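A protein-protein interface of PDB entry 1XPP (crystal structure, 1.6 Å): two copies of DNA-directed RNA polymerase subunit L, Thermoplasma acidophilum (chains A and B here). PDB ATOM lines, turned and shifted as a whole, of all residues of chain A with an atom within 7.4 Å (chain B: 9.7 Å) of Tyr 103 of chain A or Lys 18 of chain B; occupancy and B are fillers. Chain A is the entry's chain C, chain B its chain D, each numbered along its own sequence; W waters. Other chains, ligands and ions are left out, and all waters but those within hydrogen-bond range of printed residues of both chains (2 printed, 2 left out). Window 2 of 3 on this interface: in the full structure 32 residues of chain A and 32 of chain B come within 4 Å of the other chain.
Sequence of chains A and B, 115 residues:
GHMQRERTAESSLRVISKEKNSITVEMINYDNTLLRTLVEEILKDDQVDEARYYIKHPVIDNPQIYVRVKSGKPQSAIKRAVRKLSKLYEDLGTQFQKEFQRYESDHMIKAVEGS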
ATOM      1  N   GLN A  97      19.544   6.531  14.225  1.00  0.00           N
ATOM      2  CA  GLN A  97      19.751   7.707  13.395  1.00  0.00           C
ATOM      3  C   GLN A  97      20.488   8.762  14.206  1.00  0.00           C
ATOM      4  O   GLN A  97      21.455   9.342  13.707  1.00  0.00           O
ATOM      5  CB  GLN A  97      18.441   8.245  12.858  1.00  0.00           C
ATOM      6  CG  GLN A  97      18.647   9.380  11.828  1.00  0.00           C
ATOM      7  CD  GLN A  97      17.333   9.804  11.195  1.00  0.00           C
ATOM      8  OE1 GLN A  97      16.427  10.263  11.885  1.00  0.00           O
ATOM      9  NE2 GLN A  97      17.234   9.677   9.885  1.00  0.00           N
ATOM     10  N   LYS A  98      20.093   8.965  15.458  1.00  0.00           N
ATOM     11  CA  LYS A  98      20.769   9.958  16.317  1.00  0.00           C
ATOM     12  C   LYS A  98      22.194   9.519  16.634  1.00  0.00           C
ATOM     13  O   LYS A  98      23.120  10.324  16.662  1.00  0.00           O
ATOM     14  CB  LYS A  98      20.021  10.167  17.626  1.00  0.00           C
ATOM     15  CG  LYS A  98      18.752  10.988  17.527  1.00  0.00           C
ATOM     16  CD  LYS A  98      18.208  11.189  18.933  1.00  0.00           C
ATOM     17  CE  LYS A  98      16.994  12.097  18.935  1.00  0.00           C
ATOM     18  NZ  LYS A  98      16.948  12.863  20.229  1.00  0.00           N
ATOM     19  N   GLU A  99      22.374   8.229  16.890  1.00  0.00           N
ATOM     20  CA  GLU A  99      23.710   7.779  17.260  1.00  0.00           C
ATOM     21  C   GLU A  99      24.658   7.852  16.073  1.00  0.00           C
ATOM     22  O   GLU A  99      25.811   8.283  16.235  1.00  0.00           O
ATOM     23  CB  GLU A  99      23.672   6.384  17.872  1.00  0.00           C
ATOM     24  CG  GLU A  99      25.038   5.750  18.001  1.00  0.00           C
ATOM     25  CD  GLU A  99      25.945   6.411  19.024  1.00  0.00           C
ATOM     26  OE1 GLU A  99      25.490   7.302  19.791  1.00  0.00           O
ATOM     27  OE2 GLU A  99      27.141   6.013  19.031  1.00  0.00           O
ATOM     28  N   PHE A 100      24.178   7.476  14.890  1.00  0.00           N
ATOM     29  CA  PHE A 100      24.967   7.559  13.663  1.00  0.00           C
ATOM     30  C   PHE A 100      25.304   9.027  13.364  1.00  0.00           C
ATOM     31  O   PHE A 100      26.434   9.334  13.005  1.00  0.00           O
ATOM     32  CB  PHE A 100      24.254   6.934  12.466  1.00  0.00           C
ATOM     33  CG  PHE A 100      24.061   5.431  12.560  1.00  0.00           C
ATOM     34  CD1 PHE A 100      24.935   4.632  13.289  1.00  0.00           C
ATOM     35  CD2 PHE A 100      23.003   4.822  11.866  1.00  0.00           C
ATOM     36  CE1 PHE A 100      24.738   3.260  13.344  1.00  0.00           C
ATOM     37  CE2 PHE A 100      22.794   3.458  11.926  1.00  0.00           C
ATOM     38  CZ  PHE A 100      23.657   2.666  12.657  1.00  0.00           C
ATOM     39  N   GLN A 101      24.342   9.927  13.567  1.00  0.00           N
ATOM     40  CA  GLN A 101      24.590  11.374  13.414  1.00  0.00           C
ATOM     41  C   GLN A 101      25.711  11.854  14.334  1.00  0.00           C
ATOM     42  O   GLN A 101      26.586  12.623  13.921  1.00  0.00           O
ATOM     43  CB  GLN A 101      23.329  12.183  13.708  1.00  0.00           C
ATOM     44  CG  GLN A 101      22.302  12.221  12.581  1.00  0.00           C
ATOM     45  CD  GLN A 101      20.927  12.712  13.042  1.00  0.00           C
ATOM     46  OE1 GLN A 101      20.748  13.178  14.179  1.00  0.00           O
ATOM     47  NE2 GLN A 101      19.945  12.593  12.160  1.00  0.00           N
ATOM     48  N   ARG A 102      25.680  11.394  15.579  1.00  0.00           N
ATOM     49  CA  ARG A 102      26.649  11.798  16.582  1.00  0.00           C
ATOM     50  C   ARG A 102      28.021  11.204  16.287  1.00  0.00           C
ATOM     51  O   ARG A 102      29.022  11.925  16.284  1.00  0.00           O
ATOM     52  CB  ARG A 102      26.170  11.373  17.969  1.00  0.00           C
ATOM     53  CG  ARG A 102      27.034  11.852  19.096  1.00  0.00           C
ATOM     54  CD  ARG A 102      26.506  11.310  20.399  1.00  0.00           C
ATOM     55  NE  ARG A 102      27.564  11.106  21.387  1.00  0.00           N
ATOM     56  CZ  ARG A 102      28.517  10.176  21.305  1.00  0.00           C
ATOM     57  NH1 ARG A 102      28.578   9.341  20.264  1.00  0.00           N
ATOM     58  NH2 ARG A 102      29.413  10.082  22.273  1.00  0.00           N
ATOM     59  N   TYR A 103      28.065   9.898  16.022  1.00  0.00           N
ATOM     60  CA  TYR A 103      29.326   9.231  15.733  1.00  0.00           C
ATOM     61  C   TYR A 103      30.043   9.841  14.524  1.00  0.00           C
ATOM     62  O   TYR A 103      31.258  10.063  14.573  1.00  0.00           O
ATOM     63  CB  TYR A 103      29.138   7.719  15.560  1.00  0.00           C
ATOM     64  CG  TYR A 103      30.437   6.994  15.274  1.00  0.00           C
ATOM     65  CD1 TYR A 103      30.852   6.756  13.963  1.00  0.00           C
ATOM     66  CD2 TYR A 103      31.259   6.565  16.313  1.00  0.00           C
ATOM     67  CE1 TYR A 103      32.050   6.103  13.695  1.00  0.00           C
ATOM     68  CE2 TYR A 103      32.456   5.906  16.055  1.00  0.00           C
ATOM     69  CZ  TYR A 103      32.844   5.682  14.747  1.00  0.00           C
ATOM     70  OH  TYR A 103      34.032   5.034  14.493  1.00  0.00           O
ATOM     71  N   GLU A 104      29.289  10.121  13.462  1.00  0.00           N
ATOM     72  CA  GLU A 104      29.840  10.716  12.244  1.00  0.00           C
ATOM     73  C   GLU A 104      30.254  12.170  12.471  1.00  0.00           C
ATOM     74  O   GLU A 104      31.246  12.640  11.902  1.00  0.00           O
ATOM     75  CB  GLU A 104      28.836  10.621  11.095  1.00  0.00           C
ATOM     76  CG  GLU A 104      28.642   9.209  10.559  1.00  0.00           C
ATOM     77  CD  GLU A 104      27.344   9.034   9.790  1.00  0.00           C
ATOM     78  OE1 GLU A 104      27.052   9.850   8.889  1.00  0.00           O
ATOM     79  OE2 GLU A 104      26.617   8.060  10.084  1.00  0.00           O
ATOM     80  N   SER A 105      29.486  12.883  13.296  1.00  0.00           N
ATOM     81  CA  SER A 105      29.813  14.268  13.668  1.00  0.00           C
ATOM     82  C   SER A 105      31.162  14.288  14.376  1.00  0.00           C
ATOM     83  O   SER A 105      31.993  15.173  14.143  1.00  0.00           O
ATOM     84  CB  SER A 105      28.758  14.863  14.608  1.00  0.00           C
ATOM     85  OG  SER A 105      27.541  15.138  13.938  1.00  0.00           O
ATOM     86  N   ASP A 106      31.358  13.295  15.241  1.00  0.00           N
ATOM     87  CA  ASP A 106      32.589  13.116  15.987  1.00  0.00           C
ATOM     88  C   ASP A 106      33.764  12.836  15.053  1.00  0.00           C
ATOM     89  O   ASP A 106      34.825  13.450  15.195  1.00  0.00           O
ATOM     90  CB  ASP A 106      32.419  11.995  17.014  1.00  0.00           C
ATOM     91  CG  ASP A 106      31.301  12.274  18.007  1.00  0.00           C
ATOM     92  OD1 ASP A 106      31.021  13.464  18.267  1.00  0.00           O
ATOM     93  OD2 ASP A 106      30.696  11.305  18.523  1.00  0.00           O
ATOM     94  N   HIS A 107      33.561  11.923  14.099  1.00  0.00           N
ATOM     95  CA  HIS A 107      34.562  11.625  13.069  1.00  0.00           C
ATOM     96  C   HIS A 107      34.483  12.592  11.899  1.00  0.00           C
ATOM     97  O   HIS A 107      35.490  13.179  11.503  1.00  0.00           O
ATOM     98  CB  HIS A 107      34.425  10.189  12.564  1.00  0.00           C
ATOM     99  CG  HIS A 107      35.152   9.189  13.405  1.00  0.00           C
ATOM    100  ND1 HIS A 107      34.524   8.427  14.367  1.00  0.00           N
ATOM    101  CD2 HIS A 107      36.461   8.843  13.443  1.00  0.00           C
ATOM    102  CE1 HIS A 107      35.414   7.644  14.951  1.00  0.00           C
ATOM    103  NE2 HIS A 107      36.598   7.882  14.415  1.00  0.00           N
ATOM    104  N   LEU B  13      21.909   2.731  22.744  1.00  0.00           N
ATOM    105  CA  LEU B  13      22.953   2.097  21.931  1.00  0.00           C
ATOM    106  C   LEU B  13      24.078   3.052  21.627  1.00  0.00           C
ATOM    107  O   LEU B  13      23.903   4.280  21.759  1.00  0.00           O
ATOM    108  CB  LEU B  13      22.361   1.520  20.645  1.00  0.00           C
ATOM    109  CG  LEU B  13      21.447   2.430  19.816  1.00  0.00           C
ATOM    110  CD1 LEU B  13      22.275   3.400  18.953  1.00  0.00           C
ATOM    111  CD2 LEU B  13      20.459   1.631  18.942  1.00  0.00           C
ATOM    112  N   ARG B  14      25.206   2.490  21.184  1.00  0.00           N
ATOM    113  CA  ARG B  14      26.440   3.270  21.004  1.00  0.00           C
ATOM    114  C   ARG B  14      27.265   2.537  19.988  1.00  0.00           C
ATOM    115  O   ARG B  14      27.478   1.328  20.127  1.00  0.00           O
ATOM    116  CB  ARG B  14      27.215   3.317  22.326  1.00  0.00           C
ATOM    117  CG  ARG B  14      28.538   4.112  22.306  1.00  0.00           C
ATOM    118  CD  ARG B  14      28.260   5.587  22.400  1.00  0.00           C
ATOM    119  NE  ARG B  14      29.450   6.435  22.495  1.00  0.00           N
ATOM    120  CZ  ARG B  14      30.267   6.712  21.479  1.00  0.00           C
ATOM    121  NH1 ARG B  14      30.058   6.171  20.285  1.00  0.00           N
ATOM    122  NH2 ARG B  14      31.298   7.544  21.665  1.00  0.00           N
ATOM    123  N   VAL B  15      27.752   3.246  18.984  1.00  0.00           N
ATOM    124  CA  VAL B  15      28.727   2.671  18.058  1.00  0.00           C
ATOM    125  C   VAL B  15      30.048   2.521  18.809  1.00  0.00           C
ATOM    126  O   VAL B  15      30.538   3.483  19.389  1.00  0.00           O
ATOM    127  CB  VAL B  15      28.933   3.551  16.800  1.00  0.00           C
ATOM    128  CG1 VAL B  15      30.101   3.040  15.965  1.00  0.00           C
ATOM    129  CG2 VAL B  15      27.631   3.559  15.943  1.00  0.00           C
ATOM    130  N   ILE B  16      30.633   1.324  18.811  1.00  0.00           N
ATOM    131  CA  ILE B  16      31.870   1.144  19.579  1.00  0.00           C
ATOM    132  C   ILE B  16      33.078   0.715  18.759  1.00  0.00           C
ATOM    133  O   ILE B  16      34.206   0.650  19.299  1.00  0.00           O
ATOM    134  CB  ILE B  16      31.669   0.223  20.764  1.00  0.00           C
ATOM    135  CG1 ILE B  16      31.275  -1.175  20.276  1.00  0.00           C
ATOM    136  CG2 ILE B  16      30.676   0.864  21.775  1.00  0.00           C
ATOM    137  CD1 ILE B  16      31.250  -2.170  21.369  1.00  0.00           C
ATOM    138  N   SER B  17      32.861   0.440  17.477  1.00  0.00           N
ATOM    139  CA  SER B  17      33.929   0.145  16.550  1.00  0.00           C
ATOM    140  C   SER B  17      33.391   0.374  15.161  1.00  0.00           C
ATOM    141  O   SER B  17      32.222   0.119  14.892  1.00  0.00           O
ATOM    142  CB  SER B  17      34.412  -1.307  16.704  1.00  0.00           C
ATOM    143  OG  SER B  17      35.650  -1.470  16.045  1.00  0.00           O
ATOM    144  N   LYS B  18      34.268   0.864  14.302  1.00  0.00           N
ATOM    145  CA  LYS B  18      33.952   1.183  12.940  1.00  0.00           C
ATOM    146  C   LYS B  18      35.235   0.889  12.173  1.00  0.00           C
ATOM    147  O   LYS B  18      36.317   1.340  12.561  1.00  0.00           O
ATOM    148  CB  LYS B  18      33.558   2.660  12.856  1.00  0.00           C
ATOM    149  CG  LYS B  18      33.089   3.157  11.496  1.00  0.00           C
ATOM    150  CD  LYS B  18      31.642   2.773  11.198  1.00  0.00           C
ATOM    151  CE  LYS B  18      31.086   3.562  10.018  1.00  0.00           C
ATOM    152  NZ  LYS B  18      31.993   3.590   8.844  1.00  0.00           N
ATOM    153  N   GLU B  19      35.116   0.067  11.135  1.00  0.00           N
ATOM    154  CA  GLU B  19      36.246  -0.218  10.234  1.00  0.00           C
ATOM    155  C   GLU B  19      35.707  -0.098   8.825  1.00  0.00           C
ATOM    156  O   GLU B  19      34.545   0.273   8.662  1.00  0.00           O
ATOM    157  CB  GLU B  19      36.881  -1.594  10.509  1.00  0.00           C
ATOM    158  CG  GLU B  19      37.426  -1.800  11.933  1.00  0.00           C
ATOM    159  CD  GLU B  19      38.760  -1.097  12.208  1.00  0.00           C
ATOM    160  OE1 GLU B  19      39.711  -1.267  11.404  1.00  0.00           O
ATOM    161  OE2 GLU B  19      38.866  -0.388  13.244  1.00  0.00           O
ATOM    162  N   LYS B  20      36.540  -0.407   7.829  1.00  0.00           N
ATOM    163  CA  LYS B  20      36.219  -0.226   6.409  1.00  0.00           C
ATOM    164  C   LYS B  20      34.742  -0.420   6.061  1.00  0.00           C
ATOM    165  O   LYS B  20      34.028   0.547   5.767  1.00  0.00           O
ATOM    166  CB  LYS B  20      37.095  -1.143   5.541  1.00  0.00           C
ATOM    167  CG  LYS B  20      38.564  -0.731   5.473  1.00  0.00           C
ATOM    168  CD  LYS B  20      39.158  -1.055   4.113  1.00  0.00           C
ATOM    169  CE  LYS B  20      40.672  -0.925   4.106  1.00  0.00           C
ATOM    170  NZ  LYS B  20      41.244  -1.522   2.858  1.00  0.00           N
ATOM    171  N   ASN B  21      34.299  -1.668   6.109  1.00  0.00           N
ATOM    172  CA  ASN B  21      32.961  -2.038   5.731  1.00  0.00           C
ATOM    173  C   ASN B  21      32.267  -2.698   6.886  1.00  0.00           C
ATOM    174  O   ASN B  21      31.455  -3.592   6.683  1.00  0.00           O
ATOM    175  CB  ASN B  21      33.019  -3.037   4.585  1.00  0.00           C
ATOM    176  CG  ASN B  21      33.826  -2.523   3.410  1.00  0.00           C
ATOM    177  OD1 ASN B  21      33.737  -1.344   3.045  1.00  0.00           O
ATOM    178  ND2 ASN B  21      34.650  -3.395   2.835  1.00  0.00           N
ATOM    179  N   SER B  22      32.580  -2.261   8.094  1.00  0.00           N
ATOM    180  CA  SER B  22      31.969  -2.901   9.261  1.00  0.00           C
ATOM    181  C   SER B  22      31.700  -1.947  10.410  1.00  0.00           C
ATOM    182  O   SER B  22      32.272  -0.845  10.513  1.00  0.00           O
ATOM    183  CB  SER B  22      32.790  -4.102   9.722  1.00  0.00           C
ATOM    184  OG  SER B  22      33.945  -3.647  10.373  1.00  0.00           O
ATOM    185  N   ILE B  23      30.814  -2.381  11.305  1.00  0.00           N
ATOM    186  CA  ILE B  23      30.480  -1.568  12.447  1.00  0.00           C
ATOM    187  C   ILE B  23      30.067  -2.503  13.563  1.00  0.00           C
ATOM    188  O   ILE B  23      29.528  -3.605  13.311  1.00  0.00           O
ATOM    189  CB  ILE B  23      29.343  -0.551  12.091  1.00  0.00           C
ATOM    190  CG1 ILE B  23      29.267   0.564  13.116  1.00  0.00           C
ATOM    191  CG2 ILE B  23      27.988  -1.277  11.889  1.00  0.00           C
ATOM    192  CD1 ILE B  23      28.361   1.765  12.679  1.00  0.00           C
ATOM    193  N   THR B  24      30.374  -2.080  14.785  1.00  0.00           N
ATOM    194  CA  THR B  24      29.934  -2.776  15.983  1.00  0.00           C
ATOM    195  C   THR B  24      29.211  -1.797  16.878  1.00  0.00           C
ATOM    196  O   THR B  24      29.690  -0.683  17.103  1.00  0.00           O
ATOM    197  CB  THR B  24      31.144  -3.333  16.758  1.00  0.00           C
ATOM    198  OG1 THR B  24      31.905  -4.127  15.855  1.00  0.00           O
ATOM    199  CG2 THR B  24      30.690  -4.157  17.976  1.00  0.00           C
ATOM    200  N   VAL B  25      28.042  -2.222  17.348  1.00  0.00           N
ATOM    201  CA  VAL B  25      27.184  -1.408  18.168  1.00  0.00           C
ATOM    202  C   VAL B  25      26.887  -2.126  19.474  1.00  0.00           C
ATOM    203  O   VAL B  25      26.519  -3.308  19.476  1.00  0.00           O
ATOM    204  CB  VAL B  25      25.845  -1.091  17.418  1.00  0.00           C
ATOM    205  CG1 VAL B  25      24.988  -0.156  18.230  1.00  0.00           C
ATOM    206  CG2 VAL B  25      26.131  -0.503  16.065  1.00  0.00           C
ATOM    207  N   ILE B  65      26.135  -5.950  18.541  1.00  0.00           N
ATOM    208  CA  ILE B  65      25.922  -6.469  17.200  1.00  0.00           C
ATOM    209  C   ILE B  65      27.045  -5.995  16.288  1.00  0.00           C
ATOM    210  O   ILE B  65      27.585  -4.907  16.468  1.00  0.00           O
ATOM    211  CB  ILE B  65      24.512  -6.095  16.617  1.00  0.00           C
ATOM    212  CG1 ILE B  65      24.349  -4.589  16.440  1.00  0.00           C
ATOM    213  CG2 ILE B  65      23.404  -6.656  17.469  1.00  0.00           C
ATOM    214  CD1 ILE B  65      23.185  -4.210  15.519  1.00  0.00           C
ATOM    215  N   TYR B  66      27.420  -6.868  15.341  1.00  0.00           N
ATOM    216  CA  TYR B  66      28.493  -6.629  14.399  1.00  0.00           C
ATOM    217  C   TYR B  66      27.944  -6.870  12.983  1.00  0.00           C
ATOM    218  O   TYR B  66      27.289  -7.886  12.725  1.00  0.00           O
ATOM    219  CB  TYR B  66      29.602  -7.655  14.638  1.00  0.00           C
ATOM    220  CG  TYR B  66      30.635  -7.721  13.539  1.00  0.00           C
ATOM    221  CD1 TYR B  66      31.445  -6.615  13.244  1.00  0.00           C
ATOM    222  CD2 TYR B  66      30.769  -8.858  12.779  1.00  0.00           C
ATOM    223  CE1 TYR B  66      32.403  -6.695  12.228  1.00  0.00           C
ATOM    224  CE2 TYR B  66      31.718  -8.940  11.769  1.00  0.00           C
ATOM    225  CZ  TYR B  66      32.517  -7.865  11.515  1.00  0.00           C
ATOM    226  OH  TYR B  66      33.439  -7.958  10.495  1.00  0.00           O
ATOM    227  N   VAL B  67      28.219  -5.931  12.090  1.00  0.00           N
ATOM    228  CA  VAL B  67      27.742  -6.042  10.714  1.00  0.00           C
ATOM    229  C   VAL B  67      28.901  -5.712   9.791  1.00  0.00           C
ATOM    230  O   VAL B  67      29.557  -4.686   9.970  1.00  0.00           O
ATOM    231  CB  VAL B  67      26.567  -5.037  10.438  1.00  0.00           C
ATOM    232  CG1 VAL B  67      26.072  -5.156   9.009  1.00  0.00           C
ATOM    233  CG2 VAL B  67      25.396  -5.266  11.415  1.00  0.00           C
ATOM    234  N   VAL B  69      29.580  -5.431   5.525  1.00  0.00           N
ATOM    235  CA  VAL B  69      28.912  -5.362   4.218  1.00  0.00           C
ATOM    236  C   VAL B  69      29.872  -5.691   3.049  1.00  0.00           C
ATOM    237  O   VAL B  69      31.087  -5.438   3.154  1.00  0.00           O
ATOM    238  CB  VAL B  69      28.246  -3.959   4.030  1.00  0.00           C
ATOM    239  CG1 VAL B  69      27.109  -3.753   5.084  1.00  0.00           C
ATOM    240  CG2 VAL B  69      29.234  -2.830   4.118  1.00  0.00           C
ATOM    241  N   GLY B  72      28.248  -0.671  -0.029  1.00  0.00           N
ATOM    242  CA  GLY B  72      27.652   0.401   0.750  1.00  0.00           C
ATOM    243  C   GLY B  72      28.264   0.520   2.130  1.00  0.00           C
ATOM    244  O   GLY B  72      29.385   0.053   2.364  1.00  0.00           O
ATOM    245  N   LYS B  73      27.517   1.133   3.039  1.00  0.00           N
ATOM    246  CA  LYS B  73      27.984   1.421   4.386  1.00  0.00           C
ATOM    247  C   LYS B  73      27.319   0.454   5.351  1.00  0.00           C
ATOM    248  O   LYS B  73      26.190   0.061   5.134  1.00  0.00           O
ATOM    249  CB  LYS B  73      27.661   2.858   4.755  1.00  0.00           C
ATOM    250  CG  LYS B  73      28.493   3.908   3.976  1.00  0.00           C
ATOM    251  CD  LYS B  73      28.042   5.328   4.248  1.00  0.00           C
ATOM    252  CE  LYS B  73      29.122   6.357   3.863  1.00  0.00           C
ATOM    253  NZ  LYS B  73      29.912   6.021   2.625  1.00  0.00           N
ATOM    254  N   PRO B  74      28.044   0.025   6.405  1.00  0.00           N
ATOM    255  CA  PRO B  74      27.413  -0.898   7.352  1.00  0.00           C
ATOM    256  C   PRO B  74      26.260  -0.247   8.138  1.00  0.00           C
ATOM    257  O   PRO B  74      25.284  -0.920   8.423  1.00  0.00           O
ATOM    258  CB  PRO B  74      28.565  -1.280   8.283  1.00  0.00           C
ATOM    259  CG  PRO B  74      29.487  -0.119   8.227  1.00  0.00           C
ATOM    260  CD  PRO B  74      29.443   0.320   6.771  1.00  0.00           C
ATOM    261  N   GLN B  75      26.382   1.034   8.489  1.00  0.00           N
ATOM    262  CA  GLN B  75      25.300   1.744   9.172  1.00  0.00           C
ATOM    263  C   GLN B  75      24.052   1.771   8.292  1.00  0.00           C
ATOM    264  O   GLN B  75      22.943   1.720   8.815  1.00  0.00           O
ATOM    265  CB  GLN B  75      25.688   3.162   9.592  1.00  0.00           C
ATOM    266  CG  GLN B  75      26.092   4.051   8.445  1.00  0.00           C
ATOM    267  CD  GLN B  75      27.590   3.986   8.135  1.00  0.00           C
ATOM    268  OE1 GLN B  75      28.243   2.982   8.400  1.00  0.00           O
ATOM    269  NE2 GLN B  75      28.129   5.063   7.555  1.00  0.00           N
ATOM    270  N   SER B  76      24.226   1.800   6.967  1.00  0.00           N
ATOM    271  CA  SER B  76      23.066   1.712   6.056  1.00  0.00           C
ATOM    272  C   SER B  76      22.335   0.370   6.094  1.00  0.00           C
ATOM    273  O   SER B  76      21.091   0.325   5.985  1.00  0.00           O
ATOM    274  CB  SER B  76      23.481   2.031   4.612  1.00  0.00           C
ATOM    275  OG  SER B  76      23.972   3.360   4.618  1.00  0.00           O
ATOM    276  N   ILE B  78      22.144  -1.593   8.674  1.00  0.00           N
ATOM    277  CA  ILE B  78      21.349  -1.555   9.904  1.00  0.00           C
ATOM    278  C   ILE B  78      20.066  -0.718   9.693  1.00  0.00           C
ATOM    279  O   ILE B  78      18.960  -1.184  10.015  1.00  0.00           O
ATOM    280  CB  ILE B  78      22.145  -1.044  11.095  1.00  0.00           C
ATOM    281  CG1 ILE B  78      23.296  -2.024  11.369  1.00  0.00           C
ATOM    282  CG2 ILE B  78      21.182  -0.809  12.298  1.00  0.00           C
ATOM    283  CD1 ILE B  78      24.290  -1.569  12.432  1.00  0.00           C
HETATM  284  O   HOH W   1      30.472   8.446  18.713  1.00  0.00           O
HETATM  285  O   HOH W   2      31.761   9.801  20.390  1.00  0.00           O
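NH2 of Arg 14 of chain B sits close to NH2 of Arg 102 of chain A (3.2 Å).
OE2 of Glu 99 of chain A lies within hydrogen-bond range of N of Val 15 of chain B, 2.8 Å away.
The guanidinium group (NH1) of Arg 14 of chain B is in salt-bridge range of the side-chain carboxylate (OE2) of Glu 99 of chain A, 3.2 Å away.
A ring nitrogen (ND1) of His 107 of chain A lies close to the side-chain hydroxyl (OH) of Tyr 103 of chain A (3.4 Å).
The backbone carbonyl oxygen of Ile 23 of chain B lies within hydrogen-bond range of the backbone NH of Val 67 of chain B.
NH1 of Arg 102 of chain A is in salt-bridge range of OE1 of Glu 99 of chain A.
The side-chain carboxylate (OD2) of Asp 106 of chain A is in salt-bridge range of the guanidinium group (NH1) of Arg 102 of chain A (3.4 Å).
CD1 of Leu 13 of chain B touches CB of Glu 99 of chain A, 3.5 Å away.
Phe 100 of chain A touches Val 15 of chain B (CE1 to CG2, 3.9 Å).
Phe 100 of chain A touches Ile 23 of chain B.
Gln 75 of chain B touches Phe 100 of chain A (O to CE2, 3.6 Å).
Val 15 of chain B touches Tyr 103 of chain A (CG1 to CE2, 3.7 Å).
Tyr 103 of chain A touches Lys 18 of chain B.
Printed residues of chain B within 4 Å of Phe 100 of chain A: Val 15 (3.9 Å), Ile 23 (3.98 Å) and Gln 75 (3.6 Å).
Printed residues of chain B within 4 Å of Arg 102 of chain A: Arg 14.
Of the printed residues of chain B, Tyr 103 of chain A touches Val 15 and Lys 18.
No residue of chain B comes within 4 Å of Asp 106 of chain A.
Printed residues of chain A within 4 Å of Arg 14 of chain B: Glu 99 (3.2 Å) and Arg 102 (3.2 Å).
Of the printed residues of chain A, Val 15 of chain B touches Glu 99, Phe 100 and Tyr 103.
Of the printed residues of chain A, Lys 18 of chain B touches Tyr 103.
Of the printed residues of chain A, Ile 23 of chain B touches Phe 100.
The nearest printed residue of chain A that does not touch Lys 18 of chain B is His 107 of chain A (5.7 Å).
The nearest printed residue of chain A that does not touch Arg 14 of chain B is Tyr 103 of chain A (4.2 Å).
Printed residues of chain A that touch a printed residue of chain B: Glu 99, Phe 100, Arg 102 and Tyr 103.
Along chain A the printed residues that touch a printed residue of chain B span positions 99 to 103.
Printed residues of chain B that touch a printed residue of chain A: Leu 13, Arg 14, Val 15, Lys 18, Ile 23 and Gln 75.
Among the printed residues, Asp or Glu carboxylates within 4 Å of a Lys or Arg side-chain nitrogen of the other chain: Glu 99 of chain A with Arg 14 of chain B (3.2 Å).
No position is printed for both chains.
Water W1 lies within hydrogen-bond range of the guanidinium group (NH1) of Arg 102 of chain A (2.6 Å), the guanidinium group (NH1) of Arg 14 of chain B (2.8 Å) and the side-chain carboxylate (OD2) of Asp 106 of chain A (2.9 Å).
Water W2 lies within hydrogen-bond range of OD2 of Asp 106 of chain A, NH2 of Arg 14 of chain B and NH2 of Arg 102 of chain A.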
